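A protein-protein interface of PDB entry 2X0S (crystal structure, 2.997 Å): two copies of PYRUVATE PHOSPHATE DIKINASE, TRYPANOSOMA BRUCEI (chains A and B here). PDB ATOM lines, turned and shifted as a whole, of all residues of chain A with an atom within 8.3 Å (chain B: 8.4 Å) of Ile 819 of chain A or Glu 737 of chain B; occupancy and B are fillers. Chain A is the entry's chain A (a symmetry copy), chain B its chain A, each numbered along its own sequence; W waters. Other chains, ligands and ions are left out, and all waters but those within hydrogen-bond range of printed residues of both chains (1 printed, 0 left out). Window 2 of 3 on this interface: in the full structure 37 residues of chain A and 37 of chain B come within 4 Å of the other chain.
The side-chain amino group of Lys 735 of chain B is in hydrogen-bond range of the backbone carbonyl oxygen of Ile 819 of chain A. The side-chain carboxylate of Glu 738 of chain B is in hydrogen-bond range of the side-chain hydroxyl of Tyr 814 of chain A, at 3.2 Å. OD1 of Asp 829 of chain A lies within salt-bridge range of NE of Arg 773 of chain B, at 2.9 Å. NH2 of Arg 773 of chain B lies within salt-bridge range of OE1 of Glu 831 of chain A (2.7 Å). The side-chain carboxylate (OE2) of Glu 831 of chain A is in hydrogen-bond range of the side-chain hydroxyl (OG) of Ser 780 of chain B, 3.4 Å away.
OE1 of Glu 738 of chain B lies within hydrogen-bond range of N of Gly 734 of chain B (2.9 Å). The backbone carbonyl oxygen (O) of Gly 734 of chain B lies within hydrogen-bond range of the guanidinium group (NH1) of Arg 773 of chain B, 2.8 Å away. The side-chain carboxylate (OE1) of Glu 738 of chain B lies within hydrogen-bond range of the backbone NH (N) of Lys 735 of chain B (2.8 Å). The side-chain hydroxyl (OG1) of Thr 777 of chain B lies within hydrogen-bond range of the backbone carbonyl oxygen (O) of Arg 773 of chain B (2.8 Å). The side-chain hydroxyl (OG) of Ser 780 of chain B sits at hydrogen-bond distance from the backbone carbonyl oxygen (O) of Thr 777 of chain B (3.0 Å). O of Tyr 814 of chain A sits at hydrogen-bond distance from N of Ile 819 of chain A.
Tyr 814 of chain A touches Ile 697 of chain B. Glu 737 of chain B touches Ile 819 of chain A (O to CD1, 3.7 Å). CB of Lys 735 of chain B touches OH of Tyr 820 of chain A, at 3.7 Å. Glu 738 of chain B touches Tyr 820 of chain A (OE1 to OH, 3.8 Å). Arg 773 of chain B touches Tyr 820 of chain A. Glu 831 of chain A touches Lys 735 of chain B. Thr 777 of chain B touches Glu 831 of chain A.
Printed residues of chain B within 4 Å of Tyr 814 of chain A: Ile 697 (3.7 Å) and Glu 738 (3.2 Å). Printed residues of chain B within 4 Å of Tyr 820 of chain A: Lys 735, Glu 738 and Arg 773. Gln 822 of chain A touches none of the printed residues of chain B. Of the printed residues of chain B, Glu 831 of chain A touches Lys 735 (3.7 Å), Arg 773 (2.7 Å), Thr 777 (3.9 Å) and Ser 780 (3.4 Å). Printed residues of chain A within 4 Å of Ile 697 of chain B: Tyr 814 (3.7 Å). Glu 737 of chain B touches just one residue of chain A: Ile 819 (3.7 Å). Printed residues of chain A within 4 Å of Glu 738 of chain B: Tyr 814 and Tyr 820. The nearest residue of chain B that does not touch Ile 819 of chain A is Glu 738 of chain B (4.04 Å).
Of the 19 printed residues of chain B, 7 touch a printed residue of chain A. Printed residues of chain A that touch a printed residue of chain B: Tyr 814, Ile 819, Tyr 820, Asp 829 and Glu 831. Among the printed residues, 12 pairs touch across the chains.
No position is printed for both chains.
Water W1 lies within hydrogen-bond range of NH1 of Arg 773 of chain B (2.6 Å), OE1 of Glu 831 of chain A (3.0 Å), N of Lys 736 of chain B (3.2 Å), OG1 of Thr 777 of chain B (3.3 Å) and OG of Ser 780 of chain B (3.5 Å).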
ATOM      1  N   PHE A 802       0.999 -27.589   1.165  1.00  0.00           N
ATOM      2  CA  PHE A 802       0.293 -27.607  -0.127  1.00  0.00           C
ATOM      3  C   PHE A 802       1.153 -28.135  -1.269  1.00  0.00           C
ATOM      4  O   PHE A 802       2.144 -27.501  -1.647  1.00  0.00           O
ATOM      5  CB  PHE A 802      -0.166 -26.206  -0.510  1.00  0.00           C
ATOM      6  CG  PHE A 802      -1.145 -25.595   0.449  1.00  0.00           C
ATOM      7  CD1 PHE A 802      -1.971 -26.390   1.234  1.00  0.00           C
ATOM      8  CD2 PHE A 802      -1.254 -24.212   0.551  1.00  0.00           C
ATOM      9  CE1 PHE A 802      -2.877 -25.811   2.117  1.00  0.00           C
ATOM     10  CE2 PHE A 802      -2.159 -23.627   1.424  1.00  0.00           C
ATOM     11  CZ  PHE A 802      -2.969 -24.423   2.210  1.00  0.00           C
ATOM     12  N   PHE A 810      -9.656 -27.229  -3.867  1.00  0.00           N
ATOM     13  CA  PHE A 810     -10.032 -26.454  -2.689  1.00  0.00           C
ATOM     14  C   PHE A 810      -9.467 -25.039  -2.647  1.00  0.00           C
ATOM     15  O   PHE A 810     -10.132 -24.125  -2.169  1.00  0.00           O
ATOM     16  CB  PHE A 810      -9.675 -27.215  -1.402  1.00  0.00           C
ATOM     17  CG  PHE A 810      -8.206 -27.517  -1.257  1.00  0.00           C
ATOM     18  CD1 PHE A 810      -7.421 -26.799  -0.380  1.00  0.00           C
ATOM     19  CD2 PHE A 810      -7.614 -28.516  -1.998  1.00  0.00           C
ATOM     20  CE1 PHE A 810      -6.079 -27.074  -0.249  1.00  0.00           C
ATOM     21  CE2 PHE A 810      -6.275 -28.793  -1.864  1.00  0.00           C
ATOM     22  CZ  PHE A 810      -5.507 -28.068  -0.993  1.00  0.00           C
ATOM     23  N   LEU A 811      -8.247 -24.847  -3.128  1.00  0.00           N
ATOM     24  CA  LEU A 811      -7.664 -23.518  -3.051  1.00  0.00           C
ATOM     25  C   LEU A 811      -8.605 -22.499  -3.674  1.00  0.00           C
ATOM     26  O   LEU A 811      -8.906 -21.474  -3.068  1.00  0.00           O
ATOM     27  CB  LEU A 811      -6.282 -23.467  -3.698  1.00  0.00           C
ATOM     28  CG  LEU A 811      -5.196 -23.221  -2.650  1.00  0.00           C
ATOM     29  CD1 LEU A 811      -3.913 -22.635  -3.247  1.00  0.00           C
ATOM     30  CD2 LEU A 811      -5.760 -22.313  -1.576  1.00  0.00           C
ATOM     31  N   HIS A 813     -11.568 -22.578  -3.857  1.00  0.00           N
ATOM     32  CA  HIS A 813     -12.656 -22.426  -2.902  1.00  0.00           C
ATOM     33  C   HIS A 813     -12.261 -21.521  -1.728  1.00  0.00           C
ATOM     34  O   HIS A 813     -13.018 -20.637  -1.323  1.00  0.00           O
ATOM     35  CB  HIS A 813     -13.105 -23.808  -2.415  1.00  0.00           C
ATOM     36  CG  HIS A 813     -14.365 -23.790  -1.606  1.00  0.00           C
ATOM     37  ND1 HIS A 813     -15.583 -23.428  -2.136  1.00  0.00           N
ATOM     38  CD2 HIS A 813     -14.595 -24.105  -0.311  1.00  0.00           C
ATOM     39  CE1 HIS A 813     -16.510 -23.510  -1.198  1.00  0.00           C
ATOM     40  NE2 HIS A 813     -15.935 -23.918  -0.080  1.00  0.00           N
ATOM     41  N   TYR A 814     -11.066 -21.741  -1.194  1.00  0.00           N
ATOM     42  CA  TYR A 814     -10.545 -20.898  -0.129  1.00  0.00           C
ATOM     43  C   TYR A 814     -10.647 -19.425  -0.505  1.00  0.00           C
ATOM     44  O   TYR A 814     -11.035 -18.588   0.312  1.00  0.00           O
ATOM     45  CB  TYR A 814      -9.093 -21.258   0.176  1.00  0.00           C
ATOM     46  CG  TYR A 814      -8.931 -22.412   1.137  1.00  0.00           C
ATOM     47  CD1 TYR A 814      -9.157 -22.243   2.492  1.00  0.00           C
ATOM     48  CD2 TYR A 814      -8.539 -23.663   0.698  1.00  0.00           C
ATOM     49  CE1 TYR A 814      -9.011 -23.286   3.382  1.00  0.00           C
ATOM     50  CE2 TYR A 814      -8.388 -24.715   1.587  1.00  0.00           C
ATOM     51  CZ  TYR A 814      -8.624 -24.520   2.926  1.00  0.00           C
ATOM     52  OH  TYR A 814      -8.473 -25.559   3.813  1.00  0.00           O
ATOM     53  N   GLY A 815     -10.300 -19.125  -1.755  1.00  0.00           N
ATOM     54  CA  GLY A 815     -10.288 -17.760  -2.247  1.00  0.00           C
ATOM     55  C   GLY A 815     -11.624 -17.078  -2.056  1.00  0.00           C
ATOM     56  O   GLY A 815     -11.681 -15.876  -1.796  1.00  0.00           O
ATOM     57  N   ASN A 816     -12.695 -17.859  -2.174  1.00  0.00           N
ATOM     58  CA  ASN A 816     -14.053 -17.333  -2.121  1.00  0.00           C
ATOM     59  C   ASN A 816     -14.501 -16.917  -0.737  1.00  0.00           C
ATOM     60  O   ASN A 816     -14.956 -15.799  -0.519  1.00  0.00           O
ATOM     61  CB  ASN A 816     -15.034 -18.361  -2.661  1.00  0.00           C
ATOM     62  CG  ASN A 816     -15.356 -18.142  -4.106  1.00  0.00           C
ATOM     63  OD1 ASN A 816     -16.255 -18.779  -4.649  1.00  0.00           O
ATOM     64  ND2 ASN A 816     -14.630 -17.228  -4.744  1.00  0.00           N
ATOM     65  N   LEU A 817     -14.392 -17.840   0.199  1.00  0.00           N
ATOM     66  CA  LEU A 817     -14.850 -17.595   1.553  1.00  0.00           C
ATOM     67  C   LEU A 817     -13.832 -16.725   2.248  1.00  0.00           C
ATOM     68  O   LEU A 817     -14.114 -16.127   3.284  1.00  0.00           O
ATOM     69  CB  LEU A 817     -14.994 -18.919   2.271  1.00  0.00           C
ATOM     70  CG  LEU A 817     -14.079 -19.891   1.537  1.00  0.00           C
ATOM     71  CD1 LEU A 817     -12.707 -19.804   2.142  1.00  0.00           C
ATOM     72  CD2 LEU A 817     -14.623 -21.308   1.577  1.00  0.00           C
ATOM     73  N   GLY A 818     -12.642 -16.658   1.660  1.00  0.00           N
ATOM     74  CA  GLY A 818     -11.626 -15.725   2.106  1.00  0.00           C
ATOM     75  C   GLY A 818     -10.784 -16.207   3.267  1.00  0.00           C
ATOM     76  O   GLY A 818     -10.693 -15.548   4.309  1.00  0.00           O
ATOM     77  N   ILE A 819     -10.172 -17.370   3.093  1.00  0.00           N
ATOM     78  CA  ILE A 819      -9.140 -17.797   4.013  1.00  0.00           C
ATOM     79  C   ILE A 819      -7.919 -16.994   3.608  1.00  0.00           C
ATOM     80  O   ILE A 819      -7.598 -15.984   4.229  1.00  0.00           O
ATOM     81  CB  ILE A 819      -8.861 -19.298   3.906  1.00  0.00           C
ATOM     82  CG1 ILE A 819     -10.160 -20.080   4.050  1.00  0.00           C
ATOM     83  CG2 ILE A 819      -7.888 -19.721   4.978  1.00  0.00           C
ATOM     84  CD1 ILE A 819     -10.938 -19.723   5.260  1.00  0.00           C
ATOM     85  N   TYR A 820      -7.263 -17.423   2.539  1.00  0.00           N
ATOM     86  CA  TYR A 820      -6.191 -16.634   1.956  1.00  0.00           C
ATOM     87  C   TYR A 820      -6.808 -15.619   0.979  1.00  0.00           C
ATOM     88  O   TYR A 820      -7.601 -15.986   0.111  1.00  0.00           O
ATOM     89  CB  TYR A 820      -5.148 -17.545   1.293  1.00  0.00           C
ATOM     90  CG  TYR A 820      -4.579 -18.581   2.249  1.00  0.00           C
ATOM     91  CD1 TYR A 820      -5.215 -19.800   2.435  1.00  0.00           C
ATOM     92  CD2 TYR A 820      -3.420 -18.328   2.981  1.00  0.00           C
ATOM     93  CE1 TYR A 820      -4.708 -20.751   3.317  1.00  0.00           C
ATOM     94  CE2 TYR A 820      -2.901 -19.274   3.868  1.00  0.00           C
ATOM     95  CZ  TYR A 820      -3.552 -20.488   4.032  1.00  0.00           C
ATOM     96  OH  TYR A 820      -3.069 -21.449   4.899  1.00  0.00           O
ATOM     97  N   ALA A 821      -6.477 -14.339   1.148  1.00  0.00           N
ATOM     98  CA  ALA A 821      -7.040 -13.286   0.304  1.00  0.00           C
ATOM     99  C   ALA A 821      -6.713 -13.545  -1.145  1.00  0.00           C
ATOM    100  O   ALA A 821      -7.426 -13.096  -2.037  1.00  0.00           O
ATOM    101  CB  ALA A 821      -6.516 -11.929   0.708  1.00  0.00           C
ATOM    102  N   GLN A 822      -5.635 -14.282  -1.374  1.00  0.00           N
ATOM    103  CA  GLN A 822      -5.180 -14.542  -2.723  1.00  0.00           C
ATOM    104  C   GLN A 822      -4.164 -15.657  -2.778  1.00  0.00           C
ATOM    105  O   GLN A 822      -3.183 -15.656  -2.042  1.00  0.00           O
ATOM    106  CB  GLN A 822      -4.565 -13.281  -3.293  1.00  0.00           C
ATOM    107  CG  GLN A 822      -3.767 -12.509  -2.267  1.00  0.00           C
ATOM    108  CD  GLN A 822      -3.367 -11.129  -2.759  1.00  0.00           C
ATOM    109  OE1 GLN A 822      -2.683 -10.995  -3.776  1.00  0.00           O
ATOM    110  NE2 GLN A 822      -3.790 -10.091  -2.031  1.00  0.00           N
ATOM    111  N   ASP A 823      -4.417 -16.601  -3.672  1.00  0.00           N
ATOM    112  CA  ASP A 823      -3.488 -17.677  -3.982  1.00  0.00           C
ATOM    113  C   ASP A 823      -2.062 -17.338  -3.565  1.00  0.00           C
ATOM    114  O   ASP A 823      -1.364 -16.594  -4.244  1.00  0.00           O
ATOM    115  CB  ASP A 823      -3.546 -17.974  -5.473  1.00  0.00           C
ATOM    116  CG  ASP A 823      -2.699 -19.148  -5.860  1.00  0.00           C
ATOM    117  OD1 ASP A 823      -2.207 -19.828  -4.938  1.00  0.00           O
ATOM    118  OD2 ASP A 823      -2.530 -19.386  -7.084  1.00  0.00           O
ATOM    119  N   PRO A 824      -1.624 -17.895  -2.426  1.00  0.00           N
ATOM    120  CA  PRO A 824      -0.323 -17.618  -1.827  1.00  0.00           C
ATOM    121  C   PRO A 824       0.807 -18.125  -2.668  1.00  0.00           C
ATOM    122  O   PRO A 824       1.955 -17.947  -2.288  1.00  0.00           O
ATOM    123  CB  PRO A 824      -0.360 -18.449  -0.547  1.00  0.00           C
ATOM    124  CG  PRO A 824      -1.253 -19.542  -0.880  1.00  0.00           C
ATOM    125  CD  PRO A 824      -2.345 -18.888  -1.622  1.00  0.00           C
ATOM    126  N   ASP A 829       2.179 -15.115   1.458  1.00  0.00           N
ATOM    127  CA  ASP A 829       1.421 -15.127   2.698  1.00  0.00           C
ATOM    128  C   ASP A 829       2.246 -14.339   3.674  1.00  0.00           C
ATOM    129  O   ASP A 829       3.214 -14.863   4.235  1.00  0.00           O
ATOM    130  CB  ASP A 829       1.273 -16.550   3.226  1.00  0.00           C
ATOM    131  CG  ASP A 829       0.820 -16.589   4.672  1.00  0.00           C
ATOM    132  OD1 ASP A 829       1.535 -17.176   5.507  1.00  0.00           O
ATOM    133  OD2 ASP A 829      -0.248 -16.025   4.977  1.00  0.00           O
ATOM    134  N   GLU A 831       1.538 -12.970   6.624  1.00  0.00           N
ATOM    135  CA  GLU A 831       1.343 -13.369   8.017  1.00  0.00           C
ATOM    136  C   GLU A 831       2.193 -14.578   8.431  1.00  0.00           C
ATOM    137  O   GLU A 831       2.716 -14.599   9.534  1.00  0.00           O
ATOM    138  CB  GLU A 831      -0.148 -13.626   8.316  1.00  0.00           C
ATOM    139  CG  GLU A 831      -0.456 -13.795   9.820  1.00  0.00           C
ATOM    140  CD  GLU A 831      -1.753 -14.551  10.118  1.00  0.00           C
ATOM    141  OE1 GLU A 831      -2.355 -15.119   9.183  1.00  0.00           O
ATOM    142  OE2 GLU A 831      -2.164 -14.583  11.301  1.00  0.00           O
ATOM    143  N   CYS B 693      -8.720 -30.710   7.391  1.00  0.00           N
ATOM    144  CA  CYS B 693      -9.687 -29.629   7.318  1.00  0.00           C
ATOM    145  C   CYS B 693     -10.091 -29.329   5.873  1.00  0.00           C
ATOM    146  O   CYS B 693     -11.275 -29.152   5.580  1.00  0.00           O
ATOM    147  CB  CYS B 693      -9.122 -28.377   7.989  1.00  0.00           C
ATOM    148  SG  CYS B 693      -7.370 -28.070   7.635  1.00  0.00           S
ATOM    149  N   ILE B 697     -14.025 -29.117   4.651  1.00  0.00           N
ATOM    150  CA  ILE B 697     -14.674 -27.855   4.317  1.00  0.00           C
ATOM    151  C   ILE B 697     -15.320 -27.924   2.949  1.00  0.00           C
ATOM    152  O   ILE B 697     -16.389 -27.357   2.748  1.00  0.00           O
ATOM    153  CB  ILE B 697     -13.716 -26.658   4.334  1.00  0.00           C
ATOM    154  CG1 ILE B 697     -12.472 -26.962   3.507  1.00  0.00           C
ATOM    155  CG2 ILE B 697     -13.356 -26.254   5.756  1.00  0.00           C
ATOM    156  CD1 ILE B 697     -12.089 -25.836   2.555  1.00  0.00           C
ATOM    157  N   VAL B 733      -4.772 -28.193  10.269  1.00  0.00           N
ATOM    158  CA  VAL B 733      -5.040 -26.747  10.250  1.00  0.00           C
ATOM    159  C   VAL B 733      -3.797 -25.867  10.045  1.00  0.00           C
ATOM    160  O   VAL B 733      -2.775 -26.047  10.693  1.00  0.00           O
ATOM    161  CB  VAL B 733      -5.731 -26.280  11.526  1.00  0.00           C
ATOM    162  CG1 VAL B 733      -6.030 -24.795  11.435  1.00  0.00           C
ATOM    163  CG2 VAL B 733      -6.995 -27.056  11.759  1.00  0.00           C
ATOM    164  N   GLY B 734      -3.911 -24.895   9.148  1.00  0.00           N
ATOM    165  CA  GLY B 734      -2.773 -24.104   8.722  1.00  0.00           C
ATOM    166  C   GLY B 734      -2.972 -22.635   8.982  1.00  0.00           C
ATOM    167  O   GLY B 734      -2.018 -21.929   9.308  1.00  0.00           O
ATOM    168  N   LYS B 735      -4.214 -22.178   8.850  1.00  0.00           N
ATOM    169  CA  LYS B 735      -4.544 -20.786   9.117  1.00  0.00           C
ATOM    170  C   LYS B 735      -5.731 -20.572  10.067  1.00  0.00           C
ATOM    171  O   LYS B 735      -6.761 -21.234   9.965  1.00  0.00           O
ATOM    172  CB  LYS B 735      -4.798 -20.041   7.809  1.00  0.00           C
ATOM    173  CG  LYS B 735      -4.766 -18.547   8.001  1.00  0.00           C
ATOM    174  CD  LYS B 735      -5.142 -17.786   6.774  1.00  0.00           C
ATOM    175  CE  LYS B 735      -5.217 -16.320   7.127  1.00  0.00           C
ATOM    176  NZ  LYS B 735      -5.602 -15.475   5.975  1.00  0.00           N
ATOM    177  N   LYS B 736      -5.559 -19.623  10.978  1.00  0.00           N
ATOM    178  CA  LYS B 736      -6.593 -19.181  11.909  1.00  0.00           C
ATOM    179  C   LYS B 736      -8.039 -19.357  11.440  1.00  0.00           C
ATOM    180  O   LYS B 736      -8.935 -19.564  12.252  1.00  0.00           O
ATOM    181  CB  LYS B 736      -6.355 -17.705  12.261  1.00  0.00           C
ATOM    182  CG  LYS B 736      -7.035 -17.213  13.536  1.00  0.00           C
ATOM    183  CD  LYS B 736      -8.521 -16.980  13.366  1.00  0.00           C
ATOM    184  CE  LYS B 736      -9.061 -16.068  14.463  1.00  0.00           C
ATOM    185  NZ  LYS B 736      -8.580 -14.649  14.331  1.00  0.00           N
ATOM    186  N   GLU B 737      -8.283 -19.241  10.141  1.00  0.00           N
ATOM    187  CA  GLU B 737      -9.654 -19.226   9.641  1.00  0.00           C
ATOM    188  C   GLU B 737      -9.997 -20.527   8.971  1.00  0.00           C
ATOM    189  O   GLU B 737     -11.171 -20.863   8.797  1.00  0.00           O
ATOM    190  CB  GLU B 737      -9.866 -18.066   8.676  1.00  0.00           C
ATOM    191  CG  GLU B 737      -9.888 -16.725   9.365  1.00  0.00           C
ATOM    192  CD  GLU B 737      -8.549 -16.037   9.314  1.00  0.00           C
ATOM    193  OE1 GLU B 737      -7.688 -16.502   8.534  1.00  0.00           O
ATOM    194  OE2 GLU B 737      -8.369 -15.035  10.044  1.00  0.00           O
ATOM    195  N   GLU B 738      -8.957 -21.245   8.569  1.00  0.00           N
ATOM    196  CA  GLU B 738      -9.101 -22.621   8.138  1.00  0.00           C
ATOM    197  C   GLU B 738      -9.861 -23.340   9.283  1.00  0.00           C
ATOM    198  O   GLU B 738     -10.807 -24.099   9.064  1.00  0.00           O
ATOM    199  CB  GLU B 738      -7.702 -23.205   7.888  1.00  0.00           C
ATOM    200  CG  GLU B 738      -7.610 -24.321   6.866  1.00  0.00           C
ATOM    201  CD  GLU B 738      -6.171 -24.645   6.469  1.00  0.00           C
ATOM    202  OE1 GLU B 738      -5.255 -23.860   6.806  1.00  0.00           O
ATOM    203  OE2 GLU B 738      -5.957 -25.683   5.809  1.00  0.00           O
ATOM    204  N   LEU B 739      -9.477 -23.032  10.518  1.00  0.00           N
ATOM    205  CA  LEU B 739     -10.070 -23.653  11.691  1.00  0.00           C
ATOM    206  C   LEU B 739     -11.385 -23.009  12.114  1.00  0.00           C
ATOM    207  O   LEU B 739     -12.309 -23.690  12.544  1.00  0.00           O
ATOM    208  CB  LEU B 739      -9.080 -23.580  12.855  1.00  0.00           C
ATOM    209  CG  LEU B 739      -9.610 -23.959  14.243  1.00  0.00           C
ATOM    210  CD1 LEU B 739      -9.923 -25.458  14.295  1.00  0.00           C
ATOM    211  CD2 LEU B 739      -8.636 -23.555  15.375  1.00  0.00           C
ATOM    212  N   SER B 740     -11.457 -21.691  12.011  1.00  0.00           N
ATOM    213  CA  SER B 740     -12.575 -20.947  12.569  1.00  0.00           C
ATOM    214  C   SER B 740     -13.924 -21.395  12.012  1.00  0.00           C
ATOM    215  O   SER B 740     -14.954 -21.289  12.682  1.00  0.00           O
ATOM    216  CB  SER B 740     -12.372 -19.456  12.330  1.00  0.00           C
ATOM    217  OG  SER B 740     -13.408 -18.726  12.948  1.00  0.00           O
ATOM    218  N   LEU B 741     -13.903 -21.892  10.781  1.00  0.00           N
ATOM    219  CA  LEU B 741     -15.108 -22.329  10.100  1.00  0.00           C
ATOM    220  C   LEU B 741     -15.510 -23.688  10.595  1.00  0.00           C
ATOM    221  O   LEU B 741     -16.627 -23.894  11.066  1.00  0.00           O
ATOM    222  CB  LEU B 741     -14.861 -22.414   8.596  1.00  0.00           C
ATOM    223  CG  LEU B 741     -14.614 -21.082   7.892  1.00  0.00           C
ATOM    224  CD1 LEU B 741     -14.784 -21.243   6.396  1.00  0.00           C
ATOM    225  CD2 LEU B 741     -15.564 -20.019   8.421  1.00  0.00           C
ATOM    226  N   ILE B 742     -14.578 -24.621  10.461  1.00  0.00           N
ATOM    227  CA  ILE B 742     -14.779 -25.974  10.939  1.00  0.00           C
ATOM    228  C   ILE B 742     -15.337 -25.946  12.363  1.00  0.00           C
ATOM    229  O   ILE B 742     -16.170 -26.765  12.714  1.00  0.00           O
ATOM    230  CB  ILE B 742     -13.470 -26.780  10.901  1.00  0.00           C
ATOM    231  CG1 ILE B 742     -12.838 -26.701   9.519  1.00  0.00           C
ATOM    232  CG2 ILE B 742     -13.747 -28.230  11.196  1.00  0.00           C
ATOM    233  CD1 ILE B 742     -13.564 -27.552   8.513  1.00  0.00           C
ATOM    234  N   ARG B 743     -14.897 -24.986  13.169  1.00  0.00           N
ATOM    235  CA  ARG B 743     -15.327 -24.913  14.558  1.00  0.00           C
ATOM    236  C   ARG B 743     -16.843 -24.822  14.711  1.00  0.00           C
ATOM    237  O   ARG B 743     -17.460 -25.689  15.310  1.00  0.00           O
ATOM    238  CB  ARG B 743     -14.662 -23.743  15.290  1.00  0.00           C
ATOM    239  CG  ARG B 743     -15.057 -23.655  16.768  1.00  0.00           C
ATOM    240  CD  ARG B 743     -14.328 -22.523  17.465  1.00  0.00           C
ATOM    241  NE  ARG B 743     -14.494 -22.564  18.916  1.00  0.00           N
ATOM    242  CZ  ARG B 743     -13.907 -23.457  19.708  1.00  0.00           C
ATOM    243  NH1 ARG B 743     -13.124 -24.386  19.192  1.00  0.00           N
ATOM    244  NH2 ARG B 743     -14.109 -23.427  21.017  1.00  0.00           N
ATOM    245  N   ARG B 773       3.342 -23.550   9.257  1.00  0.00           N
ATOM    246  CA  ARG B 773       2.688 -22.241   9.271  1.00  0.00           C
ATOM    247  C   ARG B 773       1.871 -22.062  10.532  1.00  0.00           C
ATOM    248  O   ARG B 773       1.770 -20.966  11.065  1.00  0.00           O
ATOM    249  CB  ARG B 773       1.753 -22.063   8.066  1.00  0.00           C
ATOM    250  CG  ARG B 773       1.046 -20.717   8.110  1.00  0.00           C
ATOM    251  CD  ARG B 773       0.182 -20.396   6.926  1.00  0.00           C
ATOM    252  NE  ARG B 773      -0.173 -18.975   6.944  1.00  0.00           N
ATOM    253  CZ  ARG B 773      -1.079 -18.442   7.760  1.00  0.00           C
ATOM    254  NH1 ARG B 773      -1.715 -19.223   8.622  1.00  0.00           N
ATOM    255  NH2 ARG B 773      -1.350 -17.140   7.723  1.00  0.00           N
ATOM    256  N   THR B 777       2.250 -19.047  13.113  1.00  0.00           N
ATOM    257  CA  THR B 777       1.039 -18.246  13.379  1.00  0.00           C
ATOM    258  C   THR B 777       0.226 -18.766  14.567  1.00  0.00           C
ATOM    259  O   THR B 777      -0.998 -18.625  14.614  1.00  0.00           O
ATOM    260  CB  THR B 777       0.114 -18.156  12.140  1.00  0.00           C
ATOM    261  OG1 THR B 777      -0.487 -19.430  11.864  1.00  0.00           O
ATOM    262  CG2 THR B 777       0.904 -17.704  10.930  1.00  0.00           C
ATOM    263  N   SER B 780      -2.581 -16.467  16.617  1.00  0.00           N
ATOM    264  CA  SER B 780      -3.896 -16.290  16.038  1.00  0.00           C
ATOM    265  C   SER B 780      -4.669 -17.604  16.100  1.00  0.00           C
ATOM    266  O   SER B 780      -5.849 -17.614  16.456  1.00  0.00           O
ATOM    267  CB  SER B 780      -3.790 -15.780  14.599  1.00  0.00           C
ATOM    268  OG  SER B 780      -3.232 -16.764  13.748  1.00  0.00           O
ATOM    269  N   ILE B 781      -4.015 -18.717  15.774  1.00  0.00           N
ATOM    270  CA  ILE B 781      -4.706 -20.011  15.834  1.00  0.00           C
ATOM    271  C   ILE B 781      -5.215 -20.344  17.243  1.00  0.00           C
ATOM    272  O   ILE B 781      -6.105 -21.158  17.424  1.00  0.00           O
ATOM    273  CB  ILE B 781      -3.835 -21.168  15.334  1.00  0.00           C
ATOM    274  CG1 ILE B 781      -3.297 -20.875  13.939  1.00  0.00           C
ATOM    275  CG2 ILE B 781      -4.642 -22.451  15.297  1.00  0.00           C
ATOM    276  CD1 ILE B 781      -2.648 -22.080  13.302  1.00  0.00           C
ATOM    277  N   GLN B 783      -6.955 -18.483  19.160  1.00  0.00           N
ATOM    278  CA  GLN B 783      -8.178 -17.805  19.531  1.00  0.00           C
ATOM    279  C   GLN B 783      -9.368 -18.681  19.233  1.00  0.00           C
ATOM    280  O   GLN B 783     -10.432 -18.549  19.860  1.00  0.00           O
ATOM    281  CB  GLN B 783      -8.296 -16.501  18.760  1.00  0.00           C
ATOM    282  CG  GLN B 783      -7.203 -15.517  19.069  1.00  0.00           C
ATOM    283  CD  GLN B 783      -6.922 -14.590  17.906  1.00  0.00           C
ATOM    284  OE1 GLN B 783      -7.762 -14.422  17.019  1.00  0.00           O
ATOM    285  NE2 GLN B 783      -5.733 -13.983  17.897  1.00  0.00           N
ATOM    286  N   LYS B 784      -9.185 -19.575  18.267  1.00  0.00           N
ATOM    287  CA  LYS B 784     -10.265 -20.466  17.861  1.00  0.00           C
ATOM    288  C   LYS B 784     -10.163 -21.883  18.456  1.00  0.00           C
ATOM    289  O   LYS B 784     -11.059 -22.705  18.262  1.00  0.00           O
ATOM    290  CB  LYS B 784     -10.377 -20.507  16.328  1.00  0.00           C
ATOM    291  CG  LYS B 784     -11.065 -19.276  15.720  1.00  0.00           C
ATOM    292  CD  LYS B 784     -12.534 -19.200  16.160  1.00  0.00           C
ATOM    293  CE  LYS B 784     -13.129 -17.807  16.019  1.00  0.00           C
ATOM    294  NZ  LYS B 784     -13.988 -17.470  17.196  1.00  0.00           N
HETATM  295  O   HOH W   1      -2.944 -17.794  10.439  1.00  0.00           O
